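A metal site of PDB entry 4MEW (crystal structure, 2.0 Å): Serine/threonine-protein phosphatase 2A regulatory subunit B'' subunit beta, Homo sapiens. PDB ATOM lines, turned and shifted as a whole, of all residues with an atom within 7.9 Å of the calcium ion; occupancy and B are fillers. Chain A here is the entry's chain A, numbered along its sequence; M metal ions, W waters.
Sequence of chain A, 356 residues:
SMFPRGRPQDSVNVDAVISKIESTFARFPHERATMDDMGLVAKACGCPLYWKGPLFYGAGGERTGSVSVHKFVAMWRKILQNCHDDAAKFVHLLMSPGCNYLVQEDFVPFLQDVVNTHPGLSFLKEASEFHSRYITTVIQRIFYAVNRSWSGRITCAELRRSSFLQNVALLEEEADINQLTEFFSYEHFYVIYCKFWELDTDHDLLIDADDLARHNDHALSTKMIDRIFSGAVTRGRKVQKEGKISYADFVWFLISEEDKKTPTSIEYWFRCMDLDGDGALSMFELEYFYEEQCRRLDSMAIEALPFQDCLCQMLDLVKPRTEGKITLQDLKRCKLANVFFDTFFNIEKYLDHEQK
The backbone NH (N) of Gly 277 sits close to the side-chain carboxylate (OD1) of Asp 274, 3.2 Å away. N of Gly 279 is in hydrogen-bond range of OD2 of Asp 274, at 2.8 Å. OG of Ser 282 sits at hydrogen-bond distance from N of Glu 285 (3.1 Å). OE2 of Glu 285 sits close to N of Leu 275, 3.3 Å away.
The nearest printed residue that does not touch the calcium ion is Ser 282 (4.4 Å).
The calcium ion is bound by O of Ala 280 (2.3 Å), water W1 (2.4 Å), OD1 of Asp 274 (2.4 Å), OD1 of Asp 276 (2.4 Å), OD1 of Asp 278 (2.4 Å), OE2 of Glu 285 (2.5 Å) and OE1 of Glu 285 (2.5 Å). The calcium ion has seven donor atoms within binding distance.
Water W1 lies within hydrogen-bond range of OD2 of Asp 278 (3.1 Å) and OD2 of Asp 276 (3.2 Å).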
ATOM      1  N   PHE A 270     -19.070  21.534 -11.146  1.00  0.00           N
ATOM      2  CA  PHE A 270     -18.923  20.174 -10.639  1.00  0.00           C
ATOM      3  C   PHE A 270     -17.626  19.537 -11.113  1.00  0.00           C
ATOM      4  O   PHE A 270     -16.886  18.948 -10.325  1.00  0.00           O
ATOM      5  CB  PHE A 270     -20.112  19.292 -11.043  1.00  0.00           C
ATOM      6  CG  PHE A 270     -20.046  17.899 -10.488  1.00  0.00           C
ATOM      7  CD1 PHE A 270     -20.602  17.605  -9.245  1.00  0.00           C
ATOM      8  CD2 PHE A 270     -19.430  16.879 -11.204  1.00  0.00           C
ATOM      9  CE1 PHE A 270     -20.542  16.317  -8.730  1.00  0.00           C
ATOM     10  CE2 PHE A 270     -19.365  15.587 -10.682  1.00  0.00           C
ATOM     11  CZ  PHE A 270     -19.932  15.314  -9.444  1.00  0.00           C
ATOM     12  N   MET A 273     -14.719  20.832  -9.211  1.00  0.00           N
ATOM     13  CA  MET A 273     -14.632  20.368  -7.829  1.00  0.00           C
ATOM     14  C   MET A 273     -14.288  18.882  -7.755  1.00  0.00           C
ATOM     15  O   MET A 273     -13.714  18.417  -6.762  1.00  0.00           O
ATOM     16  CB  MET A 273     -15.947  20.638  -7.070  1.00  0.00           C
ATOM     17  CG  MET A 273     -16.266  22.119  -6.882  1.00  0.00           C
ATOM     18  SD  MET A 273     -17.708  22.458  -5.611  1.00  0.00           S
ATOM     19  CE  MET A 273     -16.798  21.849  -4.003  1.00  0.00           C
ATOM     20  N   ASP A 274     -14.636  18.152  -8.801  1.00  0.00           N
ATOM     21  CA  ASP A 274     -14.385  16.720  -8.863  1.00  0.00           C
ATOM     22  C   ASP A 274     -12.915  16.462  -9.175  1.00  0.00           C
ATOM     23  O   ASP A 274     -12.562  16.154 -10.317  1.00  0.00           O
ATOM     24  CB  ASP A 274     -15.294  16.092  -9.928  1.00  0.00           C
ATOM     25  CG  ASP A 274     -15.228  14.575  -9.932  1.00  0.00           C
ATOM     26  OD1 ASP A 274     -14.597  14.003  -9.021  1.00  0.00           O
ATOM     27  OD2 ASP A 274     -15.823  13.971 -10.850  1.00  0.00           O
ATOM     28  N   LEU A 275     -12.078  16.568  -8.144  1.00  0.00           N
ATOM     29  CA  LEU A 275     -10.625  16.504  -8.303  1.00  0.00           C
ATOM     30  C   LEU A 275     -10.111  15.249  -9.004  1.00  0.00           C
ATOM     31  O   LEU A 275      -9.221  15.335  -9.859  1.00  0.00           O
ATOM     32  CB  LEU A 275      -9.912  16.669  -6.952  1.00  0.00           C
ATOM     33  CG  LEU A 275     -10.125  17.991  -6.212  1.00  0.00           C
ATOM     34  CD1 LEU A 275      -9.291  18.029  -4.940  1.00  0.00           C
ATOM     35  CD2 LEU A 275      -9.778  19.162  -7.113  1.00  0.00           C
ATOM     36  N   ASP A 276     -10.661  14.087  -8.676  1.00  0.00           N
ATOM     37  CA  ASP A 276     -10.182  12.861  -9.296  1.00  0.00           C
ATOM     38  C   ASP A 276     -11.070  12.411 -10.465  1.00  0.00           C
ATOM     39  O   ASP A 276     -10.879  11.319 -11.005  1.00  0.00           O
ATOM     40  CB  ASP A 276      -9.996  11.734  -8.276  1.00  0.00           C
ATOM     41  CG  ASP A 276     -11.297  11.326  -7.590  1.00  0.00           C
ATOM     42  OD1 ASP A 276     -12.378  11.779  -8.003  1.00  0.00           O
ATOM     43  OD2 ASP A 276     -11.218  10.526  -6.637  1.00  0.00           O
ATOM     44  N   GLY A 277     -12.020  13.258 -10.835  1.00  0.00           N
ATOM     45  CA  GLY A 277     -12.857  13.042 -12.004  1.00  0.00           C
ATOM     46  C   GLY A 277     -13.624  11.732 -12.028  1.00  0.00           C
ATOM     47  O   GLY A 277     -13.828  11.149 -13.097  1.00  0.00           O
ATOM     48  N   ASP A 278     -14.064  11.252 -10.854  1.00  0.00           N
ATOM     49  CA  ASP A 278     -14.772   9.979 -10.783  1.00  0.00           C
ATOM     50  C   ASP A 278     -16.302  10.110 -10.766  1.00  0.00           C
ATOM     51  O   ASP A 278     -17.011   9.125 -10.625  1.00  0.00           O
ATOM     52  CB  ASP A 278     -14.303   9.163  -9.566  1.00  0.00           C
ATOM     53  CG  ASP A 278     -14.805   9.731  -8.241  1.00  0.00           C
ATOM     54  OD1 ASP A 278     -15.193  10.919  -8.201  1.00  0.00           O
ATOM     55  OD2 ASP A 278     -14.796   8.975  -7.241  1.00  0.00           O
ATOM     56  N   GLY A 279     -16.808  11.335 -10.913  1.00  0.00           N
ATOM     57  CA  GLY A 279     -18.247  11.544 -10.983  1.00  0.00           C
ATOM     58  C   GLY A 279     -18.944  11.783  -9.659  1.00  0.00           C
ATOM     59  O   GLY A 279     -20.174  11.832  -9.590  1.00  0.00           O
ATOM     60  N   ALA A 280     -18.154  11.931  -8.588  1.00  0.00           N
ATOM     61  CA  ALA A 280     -18.695  12.243  -7.259  1.00  0.00           C
ATOM     62  C   ALA A 280     -17.774  13.184  -6.498  1.00  0.00           C
ATOM     63  O   ALA A 280     -16.556  13.085  -6.607  1.00  0.00           O
ATOM     64  CB  ALA A 280     -18.921  10.960  -6.456  1.00  0.00           C
ATOM     65  N   LEU A 281     -18.360  14.092  -5.736  1.00  0.00           N
ATOM     66  CA  LEU A 281     -17.598  14.937  -4.840  1.00  0.00           C
ATOM     67  C   LEU A 281     -17.441  14.208  -3.513  1.00  0.00           C
ATOM     68  O   LEU A 281     -18.425  13.980  -2.812  1.00  0.00           O
ATOM     69  CB  LEU A 281     -18.314  16.265  -4.605  1.00  0.00           C
ATOM     70  CG  LEU A 281     -18.656  17.044  -5.869  1.00  0.00           C
ATOM     71  CD1 LEU A 281     -19.301  18.388  -5.548  1.00  0.00           C
ATOM     72  CD2 LEU A 281     -17.413  17.239  -6.732  1.00  0.00           C
ATOM     73  N   SER A 282     -16.211  13.840  -3.171  1.00  0.00           N
ATOM     74  CA  SER A 282     -15.950  13.156  -1.919  1.00  0.00           C
ATOM     75  C   SER A 282     -15.823  14.194  -0.805  1.00  0.00           C
ATOM     76  O   SER A 282     -15.804  15.404  -1.066  1.00  0.00           O
ATOM     77  CB  SER A 282     -14.659  12.354  -2.003  1.00  0.00           C
ATOM     78  OG  SER A 282     -13.539  13.229  -2.089  1.00  0.00           O
ATOM     79  N   MET A 283     -15.737  13.743   0.437  1.00  0.00           N
ATOM     80  CA  MET A 283     -15.597  14.676   1.540  1.00  0.00           C
ATOM     81  C   MET A 283     -14.221  15.329   1.509  1.00  0.00           C
ATOM     82  O   MET A 283     -14.062  16.497   1.867  1.00  0.00           O
ATOM     83  CB  MET A 283     -15.867  13.976   2.876  1.00  0.00           C
ATOM     84  CG  MET A 283     -17.289  13.421   2.989  1.00  0.00           C
ATOM     85  SD  MET A 283     -18.690  14.799   2.839  1.00  0.00           S
ATOM     86  CE  MET A 283     -19.189  14.566   0.961  1.00  0.00           C
ATOM     87  N   PHE A 284     -13.217  14.577   1.063  1.00  0.00           N
ATOM     88  CA  PHE A 284     -11.883  15.125   0.886  1.00  0.00           C
ATOM     89  C   PHE A 284     -11.929  16.285  -0.096  1.00  0.00           C
ATOM     90  O   PHE A 284     -11.333  17.341   0.126  1.00  0.00           O
ATOM     91  CB  PHE A 284     -10.901  14.062   0.389  1.00  0.00           C
ATOM     92  CG  PHE A 284      -9.611  14.634  -0.125  1.00  0.00           C
ATOM     93  CD1 PHE A 284      -8.622  15.038   0.755  1.00  0.00           C
ATOM     94  CD2 PHE A 284      -9.390  14.794  -1.483  1.00  0.00           C
ATOM     95  CE1 PHE A 284      -7.435  15.580   0.295  1.00  0.00           C
ATOM     96  CE2 PHE A 284      -8.220  15.337  -1.957  1.00  0.00           C
ATOM     97  CZ  PHE A 284      -7.231  15.729  -1.071  1.00  0.00           C
ATOM     98  N   GLU A 285     -12.645  16.088  -1.194  1.00  0.00           N
ATOM     99  CA  GLU A 285     -12.720  17.102  -2.239  1.00  0.00           C
ATOM    100  C   GLU A 285     -13.432  18.368  -1.747  1.00  0.00           C
ATOM    101  O   GLU A 285     -12.963  19.482  -2.008  1.00  0.00           O
ATOM    102  CB  GLU A 285     -13.355  16.533  -3.522  1.00  0.00           C
ATOM    103  CG  GLU A 285     -12.377  15.644  -4.301  1.00  0.00           C
ATOM    104  CD  GLU A 285     -13.069  14.684  -5.266  1.00  0.00           C
ATOM    105  OE1 GLU A 285     -14.310  14.600  -5.266  1.00  0.00           O
ATOM    106  OE2 GLU A 285     -12.352  14.000  -6.014  1.00  0.00           O
ATOM    107  N   LYS A 325     -20.932  11.148  -0.305  1.00  0.00           N
ATOM    108  CA  LYS A 325     -20.621  11.764  -1.585  1.00  0.00           C
ATOM    109  C   LYS A 325     -21.752  12.633  -2.142  1.00  0.00           C
ATOM    110  O   LYS A 325     -22.920  12.422  -1.843  1.00  0.00           O
ATOM    111  CB  LYS A 325     -20.216  10.700  -2.615  1.00  0.00           C
ATOM    112  CG  LYS A 325     -21.354   9.813  -3.085  1.00  0.00           C
ATOM    113  CD  LYS A 325     -20.886   8.817  -4.138  1.00  0.00           C
ATOM    114  CE  LYS A 325     -22.049   8.044  -4.731  1.00  0.00           C
ATOM    115  NZ  LYS A 325     -21.624   7.171  -5.871  1.00  0.00           N
ATOM    116  N   ILE A 326     -21.375  13.615  -2.962  1.00  0.00           N
ATOM    117  CA  ILE A 326     -22.340  14.476  -3.643  1.00  0.00           C
ATOM    118  C   ILE A 326     -22.182  14.263  -5.135  1.00  0.00           C
ATOM    119  O   ILE A 326     -21.092  14.426  -5.672  1.00  0.00           O
ATOM    120  CB  ILE A 326     -22.068  15.963  -3.354  1.00  0.00           C
ATOM    121  CG1 ILE A 326     -22.030  16.245  -1.850  1.00  0.00           C
ATOM    122  CG2 ILE A 326     -23.092  16.840  -4.047  1.00  0.00           C
ATOM    123  CD1 ILE A 326     -23.337  16.012  -1.154  1.00  0.00           C
HETATM  124 CA    CA M   1     -14.284  12.798  -7.002  1.00  0.00          CA
HETATM  125  O   HOH W   1     -13.978  11.252  -5.236  1.00  0.00           O
